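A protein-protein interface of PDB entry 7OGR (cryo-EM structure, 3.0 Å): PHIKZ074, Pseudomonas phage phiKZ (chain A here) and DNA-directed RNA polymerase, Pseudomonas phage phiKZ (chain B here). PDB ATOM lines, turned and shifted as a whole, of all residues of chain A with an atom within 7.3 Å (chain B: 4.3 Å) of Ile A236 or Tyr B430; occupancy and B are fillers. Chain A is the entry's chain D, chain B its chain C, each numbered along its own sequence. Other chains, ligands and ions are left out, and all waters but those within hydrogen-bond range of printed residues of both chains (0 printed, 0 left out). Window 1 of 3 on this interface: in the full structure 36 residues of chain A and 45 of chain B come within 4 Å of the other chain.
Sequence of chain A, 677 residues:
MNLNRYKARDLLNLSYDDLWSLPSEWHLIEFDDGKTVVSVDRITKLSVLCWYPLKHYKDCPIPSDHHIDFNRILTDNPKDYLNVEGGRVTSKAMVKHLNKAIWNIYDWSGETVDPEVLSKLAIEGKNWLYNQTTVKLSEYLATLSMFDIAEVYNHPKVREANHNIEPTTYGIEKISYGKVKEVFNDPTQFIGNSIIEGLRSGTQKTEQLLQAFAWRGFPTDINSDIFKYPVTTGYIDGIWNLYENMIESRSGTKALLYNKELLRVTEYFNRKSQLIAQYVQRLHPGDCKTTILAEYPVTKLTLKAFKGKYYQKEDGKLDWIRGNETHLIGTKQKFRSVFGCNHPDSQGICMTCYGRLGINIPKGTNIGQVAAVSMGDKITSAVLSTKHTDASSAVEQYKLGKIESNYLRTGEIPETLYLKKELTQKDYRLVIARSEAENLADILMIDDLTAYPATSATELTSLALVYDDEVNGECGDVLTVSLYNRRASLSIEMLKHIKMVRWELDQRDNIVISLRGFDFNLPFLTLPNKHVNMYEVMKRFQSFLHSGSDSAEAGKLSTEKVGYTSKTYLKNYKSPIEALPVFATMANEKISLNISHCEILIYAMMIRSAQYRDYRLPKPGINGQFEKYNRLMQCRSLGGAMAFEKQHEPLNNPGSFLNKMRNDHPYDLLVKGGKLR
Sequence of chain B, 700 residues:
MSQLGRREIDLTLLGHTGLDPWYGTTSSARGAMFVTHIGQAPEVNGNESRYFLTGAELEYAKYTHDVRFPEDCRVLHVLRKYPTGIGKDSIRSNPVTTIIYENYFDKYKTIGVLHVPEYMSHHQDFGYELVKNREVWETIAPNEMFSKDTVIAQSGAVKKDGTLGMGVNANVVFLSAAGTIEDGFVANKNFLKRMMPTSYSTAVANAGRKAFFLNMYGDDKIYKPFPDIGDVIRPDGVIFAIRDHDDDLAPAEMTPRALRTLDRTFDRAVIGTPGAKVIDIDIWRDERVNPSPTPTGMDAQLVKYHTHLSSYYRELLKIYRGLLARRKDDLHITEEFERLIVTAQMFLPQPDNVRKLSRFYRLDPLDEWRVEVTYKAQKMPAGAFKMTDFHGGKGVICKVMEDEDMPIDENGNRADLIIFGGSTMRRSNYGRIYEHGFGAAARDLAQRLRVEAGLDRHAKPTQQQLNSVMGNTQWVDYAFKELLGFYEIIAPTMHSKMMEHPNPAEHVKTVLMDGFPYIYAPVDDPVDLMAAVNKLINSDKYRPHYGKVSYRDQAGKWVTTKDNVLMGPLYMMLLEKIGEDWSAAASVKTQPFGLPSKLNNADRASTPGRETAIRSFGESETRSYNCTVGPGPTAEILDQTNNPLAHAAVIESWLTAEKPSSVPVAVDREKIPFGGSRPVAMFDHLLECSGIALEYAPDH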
ATOM      1  N   LEU A 144      25.796  28.717 -14.829  1.00  0.00           N
ATOM      2  CA  LEU A 144      26.274  29.112 -16.147  1.00  0.00           C
ATOM      3  C   LEU A 144      26.004  30.595 -16.333  1.00  0.00           C
ATOM      4  O   LEU A 144      24.890  31.060 -16.076  1.00  0.00           O
ATOM      5  CB  LEU A 144      25.589  28.307 -17.257  1.00  0.00           C
ATOM      6  CG  LEU A 144      25.921  28.762 -18.680  1.00  0.00           C
ATOM      7  CD1 LEU A 144      27.349  28.386 -19.036  1.00  0.00           C
ATOM      8  CD2 LEU A 144      24.939  28.195 -19.684  1.00  0.00           C
ATOM      9  N   ILE A 149      31.491  31.075 -20.756  1.00  0.00           N
ATOM     10  CA  ILE A 149      31.744  31.010 -22.192  1.00  0.00           C
ATOM     11  C   ILE A 149      33.110  31.605 -22.517  1.00  0.00           C
ATOM     12  O   ILE A 149      33.845  31.088 -23.368  1.00  0.00           O
ATOM     13  CB  ILE A 149      30.609  31.719 -22.955  1.00  0.00           C
ATOM     14  CG1 ILE A 149      29.255  31.118 -22.574  1.00  0.00           C
ATOM     15  CG2 ILE A 149      30.809  31.620 -24.458  1.00  0.00           C
ATOM     16  CD1 ILE A 149      29.111  29.657 -22.930  1.00  0.00           C
ATOM     17  N   ALA A 150      33.490  32.671 -21.811  1.00  0.00           N
ATOM     18  CA  ALA A 150      34.740  33.382 -22.052  1.00  0.00           C
ATOM     19  C   ALA A 150      35.954  32.709 -21.419  1.00  0.00           C
ATOM     20  O   ALA A 150      37.026  33.320 -21.380  1.00  0.00           O
ATOM     21  CB  ALA A 150      34.628  34.823 -21.547  1.00  0.00           C
ATOM     22  N   TYR A 153      36.191  29.909 -24.649  1.00  0.00           N
ATOM     23  CA  TYR A 153      36.424  30.666 -25.874  1.00  0.00           C
ATOM     24  C   TYR A 153      37.828  31.258 -25.904  1.00  0.00           C
ATOM     25  O   TYR A 153      38.466  31.302 -26.962  1.00  0.00           O
ATOM     26  CB  TYR A 153      35.371  31.769 -26.002  1.00  0.00           C
ATOM     27  CG  TYR A 153      35.345  32.492 -27.334  1.00  0.00           C
ATOM     28  CD1 TYR A 153      36.105  33.641 -27.546  1.00  0.00           C
ATOM     29  CD2 TYR A 153      34.538  32.040 -28.371  1.00  0.00           C
ATOM     30  CE1 TYR A 153      36.081  34.300 -28.760  1.00  0.00           C
ATOM     31  CE2 TYR A 153      34.496  32.701 -29.585  1.00  0.00           C
ATOM     32  CZ  TYR A 153      35.265  33.832 -29.770  1.00  0.00           C
ATOM     33  OH  TYR A 153      35.235  34.483 -30.982  1.00  0.00           O
ATOM     34  N   ARG A 159      41.318  29.216 -30.151  1.00  0.00           N
ATOM     35  CA  ARG A 159      41.381  30.324 -31.099  1.00  0.00           C
ATOM     36  C   ARG A 159      42.346  30.041 -32.245  1.00  0.00           C
ATOM     37  O   ARG A 159      42.215  30.636 -33.321  1.00  0.00           O
ATOM     38  CB  ARG A 159      41.767  31.615 -30.375  1.00  0.00           C
ATOM     39  CG  ARG A 159      40.729  32.134 -29.372  1.00  0.00           C
ATOM     40  CD  ARG A 159      39.440  32.576 -30.061  1.00  0.00           C
ATOM     41  NE  ARG A 159      38.440  31.514 -30.122  1.00  0.00           N
ATOM     42  CZ  ARG A 159      37.423  31.494 -30.975  1.00  0.00           C
ATOM     43  NH1 ARG A 159      36.560  30.487 -30.956  1.00  0.00           N
ATOM     44  NH2 ARG A 159      37.279  32.472 -31.858  1.00  0.00           N
ATOM     45  N   ILE A 195      30.958  23.684 -18.299  1.00  0.00           N
ATOM     46  CA  ILE A 195      30.742  23.061 -19.599  1.00  0.00           C
ATOM     47  C   ILE A 195      31.643  21.845 -19.771  1.00  0.00           C
ATOM     48  O   ILE A 195      31.192  20.775 -20.194  1.00  0.00           O
ATOM     49  CB  ILE A 195      30.964  24.091 -20.720  1.00  0.00           C
ATOM     50  CG1 ILE A 195      30.242  25.399 -20.395  1.00  0.00           C
ATOM     51  CG2 ILE A 195      30.486  23.537 -22.054  1.00  0.00           C
ATOM     52  CD1 ILE A 195      30.717  26.575 -21.220  1.00  0.00           C
ATOM     53  N   GLN A 208      27.759  18.728 -30.418  1.00  0.00           N
ATOM     54  CA  GLN A 208      27.132  20.040 -30.353  1.00  0.00           C
ATOM     55  C   GLN A 208      28.101  21.133 -29.933  1.00  0.00           C
ATOM     56  O   GLN A 208      27.857  22.308 -30.232  1.00  0.00           O
ATOM     57  CB  GLN A 208      25.943  20.010 -29.388  1.00  0.00           C
ATOM     58  CG  GLN A 208      24.851  19.035 -29.792  1.00  0.00           C
ATOM     59  CD  GLN A 208      24.192  19.411 -31.103  1.00  0.00           C
ATOM     60  OE1 GLN A 208      23.944  20.587 -31.373  1.00  0.00           O
ATOM     61  NE2 GLN A 208      23.905  18.412 -31.929  1.00  0.00           N
ATOM     62  N   LEU A 209      29.191  20.778 -29.250  1.00  0.00           N
ATOM     63  CA  LEU A 209      30.207  21.757 -28.887  1.00  0.00           C
ATOM     64  C   LEU A 209      31.164  22.054 -30.033  1.00  0.00           C
ATOM     65  O   LEU A 209      31.773  23.133 -30.050  1.00  0.00           O
ATOM     66  CB  LEU A 209      30.997  21.268 -27.670  1.00  0.00           C
ATOM     67  CG  LEU A 209      30.263  21.292 -26.328  1.00  0.00           C
ATOM     68  CD1 LEU A 209      31.126  20.687 -25.232  1.00  0.00           C
ATOM     69  CD2 LEU A 209      29.843  22.706 -25.964  1.00  0.00           C
ATOM     70  N   GLN A 211      30.201  22.414 -33.217  1.00  0.00           N
ATOM     71  CA  GLN A 211      29.513  23.416 -34.020  1.00  0.00           C
ATOM     72  C   GLN A 211      29.357  24.750 -33.302  1.00  0.00           C
ATOM     73  O   GLN A 211      28.913  25.720 -33.926  1.00  0.00           O
ATOM     74  CB  GLN A 211      28.139  22.894 -34.442  1.00  0.00           C
ATOM     75  CG  GLN A 211      28.190  21.583 -35.205  1.00  0.00           C
ATOM     76  CD  GLN A 211      26.836  20.912 -35.296  1.00  0.00           C
ATOM     77  OE1 GLN A 211      25.931  21.209 -34.517  1.00  0.00           O
ATOM     78  NE2 GLN A 211      26.690  20.001 -36.252  1.00  0.00           N
ATOM     79  N   ALA A 212      29.706  24.824 -32.018  1.00  0.00           N
ATOM     80  CA  ALA A 212      29.613  26.054 -31.244  1.00  0.00           C
ATOM     81  C   ALA A 212      30.963  26.737 -31.064  1.00  0.00           C
ATOM     82  O   ALA A 212      31.099  27.925 -31.365  1.00  0.00           O
ATOM     83  CB  ALA A 212      28.987  25.768 -29.875  1.00  0.00           C
ATOM     84  N   PHE A 213      31.973  26.008 -30.588  1.00  0.00           N
ATOM     85  CA  PHE A 213      33.279  26.603 -30.336  1.00  0.00           C
ATOM     86  C   PHE A 213      34.224  26.502 -31.526  1.00  0.00           C
ATOM     87  O   PHE A 213      35.288  27.130 -31.505  1.00  0.00           O
ATOM     88  CB  PHE A 213      33.924  25.958 -29.107  1.00  0.00           C
ATOM     89  CG  PHE A 213      33.268  26.342 -27.812  1.00  0.00           C
ATOM     90  CD1 PHE A 213      33.542  27.567 -27.220  1.00  0.00           C
ATOM     91  CD2 PHE A 213      32.371  25.486 -27.192  1.00  0.00           C
ATOM     92  CE1 PHE A 213      32.937  27.928 -26.030  1.00  0.00           C
ATOM     93  CE2 PHE A 213      31.763  25.841 -26.000  1.00  0.00           C
ATOM     94  CZ  PHE A 213      32.047  27.063 -25.419  1.00  0.00           C
ATOM     95  N   ALA A 214      33.866  25.737 -32.555  1.00  0.00           N
ATOM     96  CA  ALA A 214      34.646  25.684 -33.785  1.00  0.00           C
ATOM     97  C   ALA A 214      33.738  25.959 -34.977  1.00  0.00           C
ATOM     98  O   ALA A 214      32.599  26.403 -34.801  1.00  0.00           O
ATOM     99  CB  ALA A 214      35.347  24.333 -33.932  1.00  0.00           C
ATOM    100  N   THR A 233      31.884  30.691 -39.365  1.00  0.00           N
ATOM    101  CA  THR A 233      31.889  30.901 -37.925  1.00  0.00           C
ATOM    102  C   THR A 233      30.970  29.896 -37.240  1.00  0.00           C
ATOM    103  O   THR A 233      30.239  29.140 -37.886  1.00  0.00           O
ATOM    104  CB  THR A 233      31.466  32.333 -37.576  1.00  0.00           C
ATOM    105  OG1 THR A 233      30.314  32.694 -38.347  1.00  0.00           O
ATOM    106  CG2 THR A 233      32.592  33.307 -37.876  1.00  0.00           C
ATOM    107  N   GLY A 234      31.023  29.895 -35.911  1.00  0.00           N
ATOM    108  CA  GLY A 234      30.245  28.991 -35.094  1.00  0.00           C
ATOM    109  C   GLY A 234      29.018  29.652 -34.501  1.00  0.00           C
ATOM    110  O   GLY A 234      28.497  30.646 -35.019  1.00  0.00           O
ATOM    111  N   TYR A 235      28.547  29.088 -33.390  1.00  0.00           N
ATOM    112  CA  TYR A 235      27.362  29.611 -32.724  1.00  0.00           C
ATOM    113  C   TYR A 235      27.683  30.590 -31.603  1.00  0.00           C
ATOM    114  O   TYR A 235      26.807  31.372 -31.219  1.00  0.00           O
ATOM    115  CB  TYR A 235      26.514  28.463 -32.167  1.00  0.00           C
ATOM    116  CG  TYR A 235      25.679  27.757 -33.209  1.00  0.00           C
ATOM    117  CD1 TYR A 235      24.811  28.468 -34.029  1.00  0.00           C
ATOM    118  CD2 TYR A 235      25.751  26.377 -33.368  1.00  0.00           C
ATOM    119  CE1 TYR A 235      24.040  27.827 -34.984  1.00  0.00           C
ATOM    120  CE2 TYR A 235      24.984  25.726 -34.320  1.00  0.00           C
ATOM    121  CZ  TYR A 235      24.132  26.457 -35.124  1.00  0.00           C
ATOM    122  OH  TYR A 235      23.369  25.814 -36.070  1.00  0.00           O
ATOM    123  N   ILE A 236      28.904  30.567 -31.067  1.00  0.00           N
ATOM    124  CA  ILE A 236      29.269  31.524 -30.025  1.00  0.00           C
ATOM    125  C   ILE A 236      29.476  32.907 -30.629  1.00  0.00           C
ATOM    126  O   ILE A 236      28.873  33.892 -30.189  1.00  0.00           O
ATOM    127  CB  ILE A 236      30.516  31.043 -29.265  1.00  0.00           C
ATOM    128  CG1 ILE A 236      30.270  29.659 -28.655  1.00  0.00           C
ATOM    129  CG2 ILE A 236      30.914  32.062 -28.208  1.00  0.00           C
ATOM    130  CD1 ILE A 236      29.437  29.662 -27.392  1.00  0.00           C
ATOM    131  N   ASP A 237      30.325  33.001 -31.649  1.00  0.00           N
ATOM    132  CA  ASP A 237      30.421  34.189 -32.490  1.00  0.00           C
ATOM    133  C   ASP A 237      29.562  33.923 -33.722  1.00  0.00           C
ATOM    134  O   ASP A 237      29.923  33.103 -34.572  1.00  0.00           O
ATOM    135  CB  ASP A 237      31.872  34.499 -32.854  1.00  0.00           C
ATOM    136  CG  ASP A 237      32.683  33.255 -33.163  1.00  0.00           C
ATOM    137  OD1 ASP A 237      32.169  32.136 -32.953  1.00  0.00           O
ATOM    138  OD2 ASP A 237      33.837  33.394 -33.618  1.00  0.00           O
ATOM    139  N   GLY A 238      28.435  34.623 -33.812  1.00  0.00           N
ATOM    140  CA  GLY A 238      27.324  34.196 -34.636  1.00  0.00           C
ATOM    141  C   GLY A 238      27.566  34.281 -36.133  1.00  0.00           C
ATOM    142  O   GLY A 238      28.601  34.734 -36.624  1.00  0.00           O
ATOM    143  N   ILE A 239      26.556  33.831 -36.872  1.00  0.00           N
ATOM    144  CA  ILE A 239      26.620  33.668 -38.318  1.00  0.00           C
ATOM    145  C   ILE A 239      25.619  34.637 -38.928  1.00  0.00           C
ATOM    146  O   ILE A 239      24.404  34.470 -38.764  1.00  0.00           O
ATOM    147  CB  ILE A 239      26.318  32.224 -38.737  1.00  0.00           C
ATOM    148  CG1 ILE A 239      27.327  31.267 -38.096  1.00  0.00           C
ATOM    149  CG2 ILE A 239      26.342  32.100 -40.238  1.00  0.00           C
ATOM    150  CD1 ILE A 239      26.765  29.908 -37.758  1.00  0.00           C
ATOM    151  N   TRP A 240      26.121  35.644 -39.639  1.00  0.00           N
ATOM    152  CA  TRP A 240      25.296  36.758 -40.087  1.00  0.00           C
ATOM    153  C   TRP A 240      25.532  37.072 -41.557  1.00  0.00           C
ATOM    154  O   TRP A 240      25.519  38.233 -41.973  1.00  0.00           O
ATOM    155  CB  TRP A 240      25.555  37.991 -39.230  1.00  0.00           C
ATOM    156  CG  TRP A 240      25.212  37.800 -37.787  1.00  0.00           C
ATOM    157  CD1 TRP A 240      23.984  37.515 -37.265  1.00  0.00           C
ATOM    158  CD2 TRP A 240      26.115  37.860 -36.677  1.00  0.00           C
ATOM    159  NE1 TRP A 240      24.064  37.405 -35.898  1.00  0.00           N
ATOM    160  CE2 TRP A 240      25.362  37.611 -35.512  1.00  0.00           C
ATOM    161  CE3 TRP A 240      27.487  38.104 -36.556  1.00  0.00           C
ATOM    162  CZ2 TRP A 240      25.936  37.600 -34.243  1.00  0.00           C
ATOM    163  CZ3 TRP A 240      28.052  38.093 -35.296  1.00  0.00           C
ATOM    164  CH2 TRP A 240      27.279  37.842 -34.156  1.00  0.00           C
ATOM    165  N   THR B  25      23.409  33.648 -33.297  1.00  0.00           N
ATOM    166  CA  THR B  25      23.940  32.799 -32.240  1.00  0.00           C
ATOM    167  C   THR B  25      22.976  31.687 -31.847  1.00  0.00           C
ATOM    168  O   THR B  25      23.403  30.701 -31.239  1.00  0.00           O
ATOM    169  CB  THR B  25      24.284  33.641 -31.011  1.00  0.00           C
ATOM    170  OG1 THR B  25      23.113  34.335 -30.565  1.00  0.00           O
ATOM    171  CG2 THR B  25      25.364  34.654 -31.349  1.00  0.00           C
ATOM    172  N   THR B 424      21.679  24.861 -22.585  1.00  0.00           N
ATOM    173  CA  THR B 424      22.113  25.840 -23.578  1.00  0.00           C
ATOM    174  C   THR B 424      23.070  25.218 -24.589  1.00  0.00           C
ATOM    175  O   THR B 424      22.985  25.503 -25.788  1.00  0.00           O
ATOM    176  CB  THR B 424      22.768  27.035 -22.882  1.00  0.00           C
ATOM    177  OG1 THR B 424      21.960  27.447 -21.774  1.00  0.00           O
ATOM    178  CG2 THR B 424      22.920  28.202 -23.846  1.00  0.00           C
ATOM    179  N   MET B 425      23.985  24.363 -24.125  1.00  0.00           N
ATOM    180  CA  MET B 425      24.878  23.669 -25.048  1.00  0.00           C
ATOM    181  C   MET B 425      24.155  22.563 -25.804  1.00  0.00           C
ATOM    182  O   MET B 425      24.552  22.214 -26.921  1.00  0.00           O
ATOM    183  CB  MET B 425      26.074  23.094 -24.292  1.00  0.00           C
ATOM    184  CG  MET B 425      26.556  23.968 -23.155  1.00  0.00           C
ATOM    185  SD  MET B 425      27.222  25.527 -23.755  1.00  0.00           S
ATOM    186  CE  MET B 425      27.084  26.529 -22.284  1.00  0.00           C
ATOM    187  N   SER B 428      21.623  24.703 -28.244  1.00  0.00           N
ATOM    188  CA  SER B 428      22.399  25.641 -29.070  1.00  0.00           C
ATOM    189  C   SER B 428      21.671  26.972 -29.277  1.00  0.00           C
ATOM    190  O   SER B 428      21.527  27.461 -30.399  1.00  0.00           O
ATOM    191  CB  SER B 428      22.793  25.012 -30.412  1.00  0.00           C
ATOM    192  OG  SER B 428      23.626  23.882 -30.221  1.00  0.00           O
ATOM    193  N   ASN B 429      21.211  27.559 -28.176  1.00  0.00           N
ATOM    194  CA  ASN B 429      20.589  28.883 -28.173  1.00  0.00           C
ATOM    195  C   ASN B 429      21.453  29.805 -27.313  1.00  0.00           C
ATOM    196  O   ASN B 429      21.205  29.984 -26.119  1.00  0.00           O
ATOM    197  CB  ASN B 429      19.133  28.810 -27.677  1.00  0.00           C
ATOM    198  CG  ASN B 429      18.963  27.893 -26.480  1.00  0.00           C
ATOM    199  OD1 ASN B 429      19.930  27.331 -25.969  1.00  0.00           O
ATOM    200  ND2 ASN B 429      17.724  27.736 -26.029  1.00  0.00           N
ATOM    201  N   TYR B 430      22.467  30.404 -27.933  1.00  0.00           N
ATOM    202  CA  TYR B 430      23.467  31.177 -27.209  1.00  0.00           C
ATOM    203  C   TYR B 430      23.162  32.669 -27.151  1.00  0.00           C
ATOM    204  O   TYR B 430      23.932  33.414 -26.539  1.00  0.00           O
ATOM    205  CB  TYR B 430      24.850  30.959 -27.829  1.00  0.00           C
ATOM    206  CG  TYR B 430      25.336  29.534 -27.720  1.00  0.00           C
ATOM    207  CD1 TYR B 430      25.937  29.074 -26.553  1.00  0.00           C
ATOM    208  CD2 TYR B 430      25.192  28.645 -28.779  1.00  0.00           C
ATOM    209  CE1 TYR B 430      26.384  27.770 -26.446  1.00  0.00           C
ATOM    210  CE2 TYR B 430      25.637  27.339 -28.681  1.00  0.00           C
ATOM    211  CZ  TYR B 430      26.231  26.907 -27.512  1.00  0.00           C
ATOM    212  OH  TYR B 430      26.673  25.610 -27.409  1.00  0.00           O
ATOM    213  N   GLY B 431      22.065  33.125 -27.763  1.00  0.00           N
ATOM    214  CA  GLY B 431      21.641  34.502 -27.574  1.00  0.00           C
ATOM    215  C   GLY B 431      21.130  34.785 -26.178  1.00  0.00           C
ATOM    216  O   GLY B 431      21.167  35.941 -25.735  1.00  0.00           O
ATOM    217  N   ARG B 432      20.655  33.745 -25.483  1.00  0.00           N
ATOM    218  CA  ARG B 432      20.255  33.852 -24.083  1.00  0.00           C
ATOM    219  C   ARG B 432      21.418  34.294 -23.203  1.00  0.00           C
ATOM    220  O   ARG B 432      21.239  35.109 -22.291  1.00  0.00           O
ATOM    221  CB  ARG B 432      19.714  32.504 -23.611  1.00  0.00           C
ATOM    222  CG  ARG B 432      19.194  32.484 -22.193  1.00  0.00           C
ATOM    223  CD  ARG B 432      18.893  31.063 -21.752  1.00  0.00           C
ATOM    224  NE  ARG B 432      17.821  30.448 -22.526  1.00  0.00           N
ATOM    225  CZ  ARG B 432      17.508  29.159 -22.465  1.00  0.00           C
ATOM    226  NH1 ARG B 432      16.516  28.679 -23.203  1.00  0.00           N
ATOM    227  NH2 ARG B 432      18.187  28.348 -21.667  1.00  0.00           N
ATOM    228  N   ILE B 433      22.621  33.784 -23.484  1.00  0.00           N
ATOM    229  CA  ILE B 433      23.803  34.115 -22.692  1.00  0.00           C
ATOM    230  C   ILE B 433      24.186  35.579 -22.880  1.00  0.00           C
ATOM    231  O   ILE B 433      24.476  36.288 -21.905  1.00  0.00           O
ATOM    232  CB  ILE B 433      24.958  33.162 -23.063  1.00  0.00           C
ATOM    233  CG1 ILE B 433      24.662  31.748 -22.560  1.00  0.00           C
ATOM    234  CG2 ILE B 433      26.289  33.647 -22.504  1.00  0.00           C
ATOM    235  CD1 ILE B 433      24.411  31.670 -21.070  1.00  0.00           C
ATOM    236  N   TYR B 434      24.154  36.065 -24.125  1.00  0.00           N
ATOM    237  CA  TYR B 434      24.493  37.461 -24.390  1.00  0.00           C
ATOM    238  C   TYR B 434      23.440  38.407 -23.828  1.00  0.00           C
ATOM    239  O   TYR B 434      23.785  39.466 -23.287  1.00  0.00           O
ATOM    240  CB  TYR B 434      24.670  37.691 -25.891  1.00  0.00           C
ATOM    241  CG  TYR B 434      25.857  36.975 -26.490  1.00  0.00           C
ATOM    242  CD1 TYR B 434      27.154  37.324 -26.133  1.00  0.00           C
ATOM    243  CD2 TYR B 434      25.682  35.961 -27.424  1.00  0.00           C
ATOM    244  CE1 TYR B 434      28.245  36.674 -26.680  1.00  0.00           C
ATOM    245  CE2 TYR B 434      26.767  35.304 -27.978  1.00  0.00           C
ATOM    246  CZ  TYR B 434      28.045  35.666 -27.602  1.00  0.00           C
ATOM    247  OH  TYR B 434      29.128  35.018 -28.150  1.00  0.00           O
ATOM    248  N   MET B 530      31.994  38.460 -28.487  1.00  0.00           N
ATOM    249  CA  MET B 530      32.889  37.953 -27.457  1.00  0.00           C
ATOM    250  C   MET B 530      34.020  38.921 -27.142  1.00  0.00           C
ATOM    251  O   MET B 530      34.545  38.893 -26.024  1.00  0.00           O
ATOM    252  CB  MET B 530      33.460  36.597 -27.870  1.00  0.00           C
ATOM    253  CG  MET B 530      32.448  35.465 -27.816  1.00  0.00           C
ATOM    254  SD  MET B 530      31.948  35.007 -26.141  1.00  0.00           S
ATOM    255  CE  MET B 530      33.524  34.975 -25.290  1.00  0.00           C
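CD2 of Leu A144 touches CD1 of Ile B433, 3.8 Å away. CE of Met B425 touches CD1 of Ile A149, at 3.8 Å. Ile B433 touches Ile A149. CG2 of Ile A149 touches SD of Met B530, at 3.9 Å. Ala A150 touches Met B530 (CA to CE, 3.8 Å). Tyr A153 touches Met B530. CB of Gln A208 touches O of Met B425 (3.6 Å). Tyr A235 touches Tyr B430. O of Ile A236 touches CG2 of Thr B25, at 3.8 Å. Gly A238 touches Thr B25.
The side-chain hydroxyl (OH) of Tyr B434 lies close to the backbone carbonyl oxygen (O) of Ile A236, at 2.3 Å. The backbone carbonyl oxygen of Tyr A235 sits close to the backbone carbonyl oxygen of Thr B25, 3.5 Å away.
Ile A236 touches just these residues of chain B: Thr B25, Tyr B430, Tyr B434 and Met B530. Printed residues of chain A within 4 Å of Ser B428: Gln A208. Printed residues of chain A within 4 Å of Thr B25: Tyr A235, Ile A236 and Gly A238.
Printed residues of chain A that touch a printed residue of chain B: Leu A144, Ile A149, Ala A150, Tyr A153, Ile A195, Gln A208, Ala A212, Tyr A235, Ile A236 and Gly A238. Hydrophobic or aromatic side chains of chain A that line the printed part of chain B: Leu A144, Ile A149, Ala A150, Tyr A153, Ile A195, Ala A212, Tyr A235 and Ile A236. Of the 11 printed residues of chain B, 8 touch a printed residue of chain A. Hydrophobic or aromatic side chains of chain B within 4 Å of the printed part of chain A: Met B425, Tyr B430, Ile B433, Tyr B434 and Met B530. Among the printed residues, 19 pairs touch across the chains. Among the printed residues, no Asp or Glu carboxylate lies within 4 Å of a Lys or Arg side-chain nitrogen of the other chain.
O of Ala A212 is in hydrogen-bond range of N of Tyr A235, 3.5 Å away. SD of Met B425 lies close to OH of Tyr B430, 3.7 Å away. The backbone carbonyl oxygen of Ala A212 lies close to the backbone NH of Ile A236 (3.4 Å). The side-chain hydroxyl of Thr A233 sits at hydrogen-bond distance from the backbone carbonyl oxygen of Gly A238, at 3.2 Å. The side-chain hydroxyl of Thr B25 is in hydrogen-bond range of the backbone NH of Gly B431 (3.2 Å). The side-chain hydroxyl (OH) of Tyr B434 sits close to the side-chain sulfur (SD) of Met B530 (3.5 Å).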
